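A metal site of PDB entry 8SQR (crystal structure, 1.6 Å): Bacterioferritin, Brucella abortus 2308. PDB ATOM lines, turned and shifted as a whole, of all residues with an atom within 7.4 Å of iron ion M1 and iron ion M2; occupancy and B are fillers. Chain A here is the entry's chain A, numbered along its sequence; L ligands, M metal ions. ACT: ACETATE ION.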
ATOM      1  N   ALA A  18      -3.935  21.679  -0.777  1.00  0.00           N
ATOM      2  CA  ALA A  18      -4.932  20.684  -0.421  1.00  0.00           C
ATOM      3  C   ALA A  18      -6.037  21.298   0.430  1.00  0.00           C
ATOM      4  O   ALA A  18      -7.219  20.982   0.248  1.00  0.00           O
ATOM      5  CB  ALA A  18      -4.261  19.530   0.319  1.00  0.00           C
ATOM      6  N   LEU A  21      -8.567  22.978  -1.713  1.00  0.00           N
ATOM      7  CA  LEU A  21      -9.434  22.025  -2.408  1.00  0.00           C
ATOM      8  C   LEU A  21     -10.431  21.401  -1.454  1.00  0.00           C
ATOM      9  O   LEU A  21     -11.615  21.221  -1.790  1.00  0.00           O
ATOM     10  CB  LEU A  21      -8.605  20.942  -3.088  1.00  0.00           C
ATOM     11  CG  LEU A  21      -7.664  21.404  -4.175  1.00  0.00           C
ATOM     12  CD1 LEU A  21      -6.846  20.236  -4.707  1.00  0.00           C
ATOM     13  CD2 LEU A  21      -8.428  22.097  -5.283  1.00  0.00           C
ATOM     14  N   GLU A  22      -9.998  21.059  -0.244  1.00  0.00           N
ATOM     15  CA  GLU A  22     -10.910  20.441   0.711  1.00  0.00           C
ATOM     16  C   GLU A  22     -12.003  21.406   1.152  1.00  0.00           C
ATOM     17  O   GLU A  22     -13.186  21.023   1.225  1.00  0.00           O
ATOM     18  CB  GLU A  22     -10.123  19.928   1.929  1.00  0.00           C
ATOM     19  CG  GLU A  22      -9.169  18.809   1.575  1.00  0.00           C
ATOM     20  CD  GLU A  22      -9.919  17.606   1.181  1.00  0.00           C
ATOM     21  OE1 GLU A  22     -11.114  17.529   1.560  1.00  0.00           O
ATOM     22  OE2 GLU A  22      -9.355  16.778   0.478  1.00  0.00           O
ATOM     23  N   LEU A  23     -11.635  22.653   1.483  1.00  0.00           N
ATOM     24  CA  LEU A  23     -12.649  23.639   1.826  1.00  0.00           C
ATOM     25  C   LEU A  23     -13.584  23.904   0.656  1.00  0.00           C
ATOM     26  O   LEU A  23     -14.780  24.138   0.856  1.00  0.00           O
ATOM     27  CB  LEU A  23     -11.980  24.933   2.271  1.00  0.00           C
ATOM     28  CG  LEU A  23     -11.192  24.791   3.581  1.00  0.00           C
ATOM     29  CD1 LEU A  23     -10.378  26.037   3.811  1.00  0.00           C
ATOM     30  CD2 LEU A  23     -12.133  24.533   4.733  1.00  0.00           C
ATOM     31  N   ALA A  25     -14.538  21.679  -1.487  1.00  0.00           N
ATOM     32  CA  ALA A  25     -15.432  20.531  -1.509  1.00  0.00           C
ATOM     33  C   ALA A  25     -16.425  20.581  -0.354  1.00  0.00           C
ATOM     34  O   ALA A  25     -17.594  20.213  -0.528  1.00  0.00           O
ATOM     35  CB  ALA A  25     -14.650  19.237  -1.445  1.00  0.00           C
ATOM     36  N   VAL A  26     -15.996  21.023   0.834  1.00  0.00           N
ATOM     37  CA  VAL A  26     -16.965  21.221   1.894  1.00  0.00           C
ATOM     38  C   VAL A  26     -18.103  22.102   1.393  1.00  0.00           C
ATOM     39  O   VAL A  26     -19.274  21.778   1.560  1.00  0.00           O
ATOM     40  CB  VAL A  26     -16.313  21.863   3.138  1.00  0.00           C
ATOM     41  CG1 VAL A  26     -17.424  22.297   4.104  1.00  0.00           C
ATOM     42  CG2 VAL A  26     -15.362  20.911   3.823  1.00  0.00           C
ATOM     43  N   TYR A  29     -20.235  20.388  -1.554  1.00  0.00           N
ATOM     44  CA  TYR A  29     -21.126  19.330  -1.081  1.00  0.00           C
ATOM     45  C   TYR A  29     -22.256  19.912  -0.223  1.00  0.00           C
ATOM     46  O   TYR A  29     -23.401  19.431  -0.281  1.00  0.00           O
ATOM     47  CB  TYR A  29     -20.326  18.261  -0.319  1.00  0.00           C
ATOM     48  CG  TYR A  29     -19.619  17.251  -1.194  1.00  0.00           C
ATOM     49  CD1 TYR A  29     -20.335  16.391  -1.991  1.00  0.00           C
ATOM     50  CD2 TYR A  29     -18.245  17.130  -1.165  1.00  0.00           C
ATOM     51  CE1 TYR A  29     -19.683  15.434  -2.796  1.00  0.00           C
ATOM     52  CE2 TYR A  29     -17.566  16.189  -1.970  1.00  0.00           C
ATOM     53  CZ  TYR A  29     -18.314  15.345  -2.781  1.00  0.00           C
ATOM     54  OH  TYR A  29     -17.675  14.397  -3.571  1.00  0.00           O
ATOM     55  N   GLU A  51     -20.954  13.538   3.057  1.00  0.00           N
ATOM     56  CA  GLU A  51     -19.666  13.711   2.387  1.00  0.00           C
ATOM     57  C   GLU A  51     -19.053  15.066   2.709  1.00  0.00           C
ATOM     58  O   GLU A  51     -17.826  15.178   2.850  1.00  0.00           O
ATOM     59  CB  GLU A  51     -19.820  13.584   0.872  1.00  0.00           C
ATOM     60  CG  GLU A  51     -20.265  12.200   0.356  1.00  0.00           C
ATOM     61  CD  GLU A  51     -19.153  11.153   0.400  1.00  0.00           C
ATOM     62  OE1 GLU A  51     -18.260  11.247   1.262  1.00  0.00           O
ATOM     63  OE2 GLU A  51     -19.182  10.228  -0.452  1.00  0.00           O
ATOM     64  N   GLU A  54     -17.393  14.771   6.007  1.00  0.00           N
ATOM     65  CA  GLU A  54     -16.112  14.071   5.899  1.00  0.00           C
ATOM     66  C   GLU A  54     -15.018  14.987   5.378  1.00  0.00           C
ATOM     67  O   GLU A  54     -13.885  14.918   5.863  1.00  0.00           O
ATOM     68  CB  GLU A  54     -16.254  12.854   4.977  1.00  0.00           C
ATOM     69  CG  GLU A  54     -17.006  11.760   5.651  1.00  0.00           C
ATOM     70  CD  GLU A  54     -16.830  10.459   4.947  1.00  0.00           C
ATOM     71  OE1 GLU A  54     -15.769  10.242   4.314  1.00  0.00           O
ATOM     72  OE2 GLU A  54     -17.762   9.663   5.029  1.00  0.00           O
ATOM     73  N   GLU A  55     -15.340  15.830   4.399  1.00  0.00           N
ATOM     74  CA  GLU A  55     -14.330  16.750   3.901  1.00  0.00           C
ATOM     75  C   GLU A  55     -13.946  17.743   4.989  1.00  0.00           C
ATOM     76  O   GLU A  55     -12.794  18.192   5.028  1.00  0.00           O
ATOM     77  CB  GLU A  55     -14.796  17.508   2.643  1.00  0.00           C
ATOM     78  CG  GLU A  55     -15.361  16.653   1.465  1.00  0.00           C
ATOM     79  CD  GLU A  55     -14.335  15.799   0.778  1.00  0.00           C
ATOM     80  OE1 GLU A  55     -13.271  15.593   1.356  1.00  0.00           O
ATOM     81  OE2 GLU A  55     -14.603  15.318  -0.346  1.00  0.00           O
ATOM     82  N   MET A  56     -14.893  18.099   5.875  1.00  0.00           N
ATOM     83  CA  MET A  56     -14.550  18.977   7.005  1.00  0.00           C
ATOM     84  C   MET A  56     -13.475  18.360   7.882  1.00  0.00           C
ATOM     85  O   MET A  56     -12.538  19.031   8.309  1.00  0.00           O
ATOM     86  CB  MET A  56     -15.802  19.256   7.842  1.00  0.00           C
ATOM     87  CG  MET A  56     -16.874  20.060   7.161  1.00  0.00           C
ATOM     88  SD  MET A  56     -18.441  20.164   8.084  1.00  0.00           S
ATOM     89  CE  MET A  56     -19.634  20.414   6.769  1.00  0.00           C
ATOM     90  N   HIS A  58     -11.230  16.208   6.881  1.00  0.00           N
ATOM     91  CA  HIS A  58      -9.987  16.300   6.106  1.00  0.00           C
ATOM     92  C   HIS A  58      -9.347  17.678   6.243  1.00  0.00           C
ATOM     93  O   HIS A  58      -8.133  17.805   6.472  1.00  0.00           O
ATOM     94  CB  HIS A  58     -10.222  16.027   4.631  1.00  0.00           C
ATOM     95  CG  HIS A  58     -10.652  14.633   4.317  1.00  0.00           C
ATOM     96  ND1 HIS A  58     -11.122  14.258   3.078  1.00  0.00           N
ATOM     97  CD2 HIS A  58     -10.697  13.520   5.089  1.00  0.00           C
ATOM     98  CE1 HIS A  58     -11.434  12.979   3.094  1.00  0.00           C
ATOM     99  NE2 HIS A  58     -11.187  12.505   4.310  1.00  0.00           N
ATOM    100  N   ALA A  59     -10.147  18.737   6.057  1.00  0.00           N
ATOM    101  CA  ALA A  59      -9.635  20.088   6.237  1.00  0.00           C
ATOM    102  C   ALA A  59      -9.022  20.273   7.622  1.00  0.00           C
ATOM    103  O   ALA A  59      -7.940  20.879   7.747  1.00  0.00           O
ATOM    104  CB  ALA A  59     -10.751  21.106   6.001  1.00  0.00           C
ATOM    105  N   LEU A  62      -5.588  18.771   7.815  1.00  0.00           N
ATOM    106  CA  LEU A  62      -4.598  19.573   7.096  1.00  0.00           C
ATOM    107  C   LEU A  62      -4.211  20.805   7.906  1.00  0.00           C
ATOM    108  O   LEU A  62      -3.029  21.159   7.993  1.00  0.00           O
ATOM    109  CB  LEU A  62      -5.127  19.965   5.704  1.00  0.00           C
ATOM    110  CG  LEU A  62      -5.185  18.846   4.669  1.00  0.00           C
ATOM    111  CD1 LEU A  62      -6.127  19.208   3.521  1.00  0.00           C
ATOM    112  CD2 LEU A  62      -3.812  18.525   4.116  1.00  0.00           C
ATOM    113  N   ASP A  94     -19.316  17.103  -8.568  1.00  0.00           N
ATOM    114  CA  ASP A  94     -18.601  16.442  -7.488  1.00  0.00           C
ATOM    115  C   ASP A  94     -17.441  15.629  -8.028  1.00  0.00           C
ATOM    116  O   ASP A  94     -16.312  15.692  -7.524  1.00  0.00           O
ATOM    117  CB  ASP A  94     -19.537  15.510  -6.723  1.00  0.00           C
ATOM    118  CG  ASP A  94     -20.657  16.226  -5.972  1.00  0.00           C
ATOM    119  OD1 ASP A  94     -20.504  17.405  -5.638  1.00  0.00           O
ATOM    120  OD2 ASP A  94     -21.690  15.550  -5.716  1.00  0.00           O
ATOM    121  N   GLY A  97     -14.405  17.549  -9.132  1.00  0.00           N
ATOM    122  CA  GLY A  97     -13.643  17.988  -7.979  1.00  0.00           C
ATOM    123  C   GLY A  97     -12.768  16.877  -7.422  1.00  0.00           C
ATOM    124  O   GLY A  97     -11.631  17.128  -7.001  1.00  0.00           O
ATOM    125  N   GLU A  98     -13.277  15.647  -7.400  1.00  0.00           N
ATOM    126  CA  GLU A  98     -12.510  14.549  -6.836  1.00  0.00           C
ATOM    127  C   GLU A  98     -11.308  14.212  -7.721  1.00  0.00           C
ATOM    128  O   GLU A  98     -10.204  13.954  -7.222  1.00  0.00           O
ATOM    129  CB  GLU A  98     -13.399  13.319  -6.629  1.00  0.00           C
ATOM    130  CG  GLU A  98     -14.591  13.508  -5.664  1.00  0.00           C
ATOM    131  CD  GLU A  98     -14.221  13.748  -4.225  1.00  0.00           C
ATOM    132  OE1 GLU A  98     -13.129  13.342  -3.840  1.00  0.00           O
ATOM    133  OE2 GLU A  98     -15.020  14.359  -3.446  1.00  0.00           O
ATOM    134  N   ALA A 101      -8.660  16.826  -7.049  1.00  0.00           N
ATOM    135  CA  ALA A 101      -7.979  16.582  -5.769  1.00  0.00           C
ATOM    136  C   ALA A 101      -7.028  15.398  -5.878  1.00  0.00           C
ATOM    137  O   ALA A 101      -5.881  15.464  -5.407  1.00  0.00           O
ATOM    138  CB  ALA A 101      -9.014  16.344  -4.672  1.00  0.00           C
ATOM    139  N   TYR A 105      -3.076  15.423  -4.972  1.00  0.00           N
ATOM    140  CA  TYR A 105      -2.478  14.662  -3.877  1.00  0.00           C
ATOM    141  C   TYR A 105      -1.417  13.678  -4.370  1.00  0.00           C
ATOM    142  O   TYR A 105      -0.445  13.415  -3.639  1.00  0.00           O
ATOM    143  CB  TYR A 105      -3.591  13.945  -3.093  1.00  0.00           C
ATOM    144  CG  TYR A 105      -4.636  14.896  -2.548  1.00  0.00           C
ATOM    145  CD1 TYR A 105      -4.360  16.258  -2.427  1.00  0.00           C
ATOM    146  CD2 TYR A 105      -5.915  14.444  -2.178  1.00  0.00           C
ATOM    147  CE1 TYR A 105      -5.307  17.147  -1.960  1.00  0.00           C
ATOM    148  CE2 TYR A 105      -6.874  15.354  -1.674  1.00  0.00           C
ATOM    149  CZ  TYR A 105      -6.528  16.697  -1.578  1.00  0.00           C
ATOM    150  OH  TYR A 105      -7.444  17.627  -1.116  1.00  0.00           O
ATOM    151  N   LEU A 127      -5.369  10.746   2.094  1.00  0.00           N
ATOM    152  CA  LEU A 127      -6.308  11.540   1.310  1.00  0.00           C
ATOM    153  C   LEU A 127      -6.514  10.943  -0.075  1.00  0.00           C
ATOM    154  O   LEU A 127      -7.643  10.879  -0.580  1.00  0.00           O
ATOM    155  CB  LEU A 127      -5.824  12.986   1.194  1.00  0.00           C
ATOM    156  CG  LEU A 127      -5.800  13.791   2.475  1.00  0.00           C
ATOM    157  CD1 LEU A 127      -5.182  15.153   2.198  1.00  0.00           C
ATOM    158  CD2 LEU A 127      -7.193  13.939   3.074  1.00  0.00           C
ATOM    159  N   ASP A 130      -8.778   8.001   0.101  1.00  0.00           N
ATOM    160  CA  ASP A 130     -10.144   8.469   0.334  1.00  0.00           C
ATOM    161  C   ASP A 130     -10.768   8.996  -0.954  1.00  0.00           C
ATOM    162  O   ASP A 130     -11.915   8.677  -1.275  1.00  0.00           O
ATOM    163  CB  ASP A 130     -10.157   9.564   1.415  1.00  0.00           C
ATOM    164  CG  ASP A 130      -9.899   9.034   2.812  1.00  0.00           C
ATOM    165  OD1 ASP A 130      -9.852   7.799   3.008  1.00  0.00           O
ATOM    166  OD2 ASP A 130      -9.740   9.868   3.730  1.00  0.00           O
ATOM    167  N   GLU A 131     -10.012   9.818  -1.709  1.00  0.00           N
ATOM    168  CA  GLU A 131     -10.555  10.374  -2.939  1.00  0.00           C
ATOM    169  C   GLU A 131     -10.884   9.274  -3.954  1.00  0.00           C
ATOM    170  O   GLU A 131     -11.889   9.366  -4.679  1.00  0.00           O
ATOM    171  CB  GLU A 131      -9.599  11.394  -3.573  1.00  0.00           C
ATOM    172  CG  GLU A 131      -9.098  12.548  -2.702  1.00  0.00           C
ATOM    173  CD  GLU A 131     -10.196  13.351  -2.069  1.00  0.00           C
ATOM    174  OE1 GLU A 131     -11.343  13.074  -2.412  1.00  0.00           O
ATOM    175  OE2 GLU A 131      -9.920  14.224  -1.220  1.00  0.00           O
ATOM    176  N   GLU A 132     -10.016   8.258  -4.088  1.00  0.00           N
ATOM    177  CA  GLU A 132     -10.358   7.171  -5.006  1.00  0.00           C
ATOM    178  C   GLU A 132     -11.620   6.444  -4.545  1.00  0.00           C
ATOM    179  O   GLU A 132     -12.427   6.022  -5.378  1.00  0.00           O
ATOM    180  CB  GLU A 132      -9.159   6.220  -5.190  1.00  0.00           C
ATOM    181  CG  GLU A 132      -8.039   6.908  -6.002  1.00  0.00           C
ATOM    182  CD  GLU A 132      -6.962   6.001  -6.604  1.00  0.00           C
ATOM    183  OE1 GLU A 132      -7.064   4.762  -6.535  1.00  0.00           O
ATOM    184  OE2 GLU A 132      -5.971   6.547  -7.162  1.00  0.00           O
ATOM    185  N   HIS A 134     -14.197   7.967  -3.040  1.00  0.00           N
ATOM    186  CA  HIS A 134     -15.267   8.862  -3.484  1.00  0.00           C
ATOM    187  C   HIS A 134     -15.479   8.757  -4.987  1.00  0.00           C
ATOM    188  O   HIS A 134     -16.618   8.819  -5.473  1.00  0.00           O
ATOM    189  CB  HIS A 134     -14.936  10.319  -3.102  1.00  0.00           C
ATOM    190  CG  HIS A 134     -14.778  10.566  -1.633  1.00  0.00           C
ATOM    191  ND1 HIS A 134     -14.181  11.706  -1.140  1.00  0.00           N
ATOM    192  CD2 HIS A 134     -15.135   9.844  -0.548  1.00  0.00           C
ATOM    193  CE1 HIS A 134     -14.168  11.670   0.183  1.00  0.00           C
ATOM    194  NE2 HIS A 134     -14.740  10.547   0.568  1.00  0.00           N
ATOM    195  N   ILE A 135     -14.389   8.662  -5.762  1.00  0.00           N
ATOM    196  CA  ILE A 135     -14.503   8.494  -7.210  1.00  0.00           C
ATOM    197  C   ILE A 135     -15.251   7.201  -7.531  1.00  0.00           C
ATOM    198  O   ILE A 135     -16.157   7.182  -8.375  1.00  0.00           O
ATOM    199  CB  ILE A 135     -13.105   8.519  -7.865  1.00  0.00           C
ATOM    200  CG1 ILE A 135     -12.518   9.946  -7.771  1.00  0.00           C
ATOM    201  CG2 ILE A 135     -13.176   8.076  -9.307  1.00  0.00           C
ATOM    202  CD1 ILE A 135     -11.019   9.969  -7.976  1.00  0.00           C
ATOM    203  N   LEU A 138     -18.966   7.803  -6.822  1.00  0.00           N
ATOM    204  CA  LEU A 138     -19.618   8.698  -7.756  1.00  0.00           C
ATOM    205  C   LEU A 138     -19.717   8.088  -9.148  1.00  0.00           C
ATOM    206  O   LEU A 138     -20.719   8.279  -9.830  1.00  0.00           O
ATOM    207  CB  LEU A 138     -18.895  10.039  -7.813  1.00  0.00           C
ATOM    208  CG  LEU A 138     -19.063  10.951  -6.618  1.00  0.00           C
ATOM    209  CD1 LEU A 138     -17.985  12.017  -6.690  1.00  0.00           C
ATOM    210  CD2 LEU A 138     -20.443  11.587  -6.614  1.00  0.00           C
HETATM  211  C   ACT L   1     -12.065  16.734  -2.611  1.00  0.00           C
HETATM  212  O   ACT L   1     -13.033  15.991  -2.864  1.00  0.00           O
HETATM  213  OXT ACT L   1     -11.274  16.589  -1.663  1.00  0.00           O
HETATM  214  CH3 ACT L   1     -11.893  17.931  -3.577  1.00  0.00           C
HETATM  215 FE    FE M   1     -13.360  13.923  -1.770  1.00  0.00          FE
HETATM  216 FE    FE M   2     -11.209  15.495   0.379  1.00  0.00          FE
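ND1 of His 58 sits close to OE1 of Glu 55 (3.1 Å). The side-chain hydroxyl (OH) of Tyr 105 lies close to the side-chain carboxylate (OE2) of Glu 22. A ring nitrogen (NE2) of His 58 sits at hydrogen-bond distance from the side-chain carboxylate (OD2) of Asp 130, 3.1 Å away. The side-chain carboxylate of Glu 98 sits close to the side-chain hydroxyl of Tyr 29 (2.7 Å).
Within 4 Å of iron ion M1: Glu 55, Glu 98, Glu 131 and His 134. The nearest printed residue that does not touch iron ion M1 is Tyr 29 (4.7 Å).
Residues that only touch iron ion M2: His 58. The nearest printed residue that does not touch iron ion M2 is Tyr 105 (4.6 Å).
Iron ion M1 is bound by OE1 of Glu 98. OE1 of Glu 131 binds iron ion M1. Iron ion M1 is bound by the side-chain carboxylate (OE2) of Glu 55, 2.3 Å away. O of the ligand binds iron ion M1. OE2 of Glu 98 is bound to iron ion M1. Iron ion M1 is bound by a ring nitrogen (ND1) of His 134 (2.4 Å). Iron ion M1 has six donor atoms within binding distance.
Iron ion M2 is bound by the side-chain carboxylate (OE2) of Glu 22 (2.3 Å), the side-chain carboxylate (OE1) of Glu 55 (2.3 Å), an oxygen (OXT) of the ligand (2.3 Å), the side-chain carboxylate (OE1) of Glu 22 (2.4 Å) and the side-chain carboxylate (OE2) of Glu 131 (2.4 Å).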
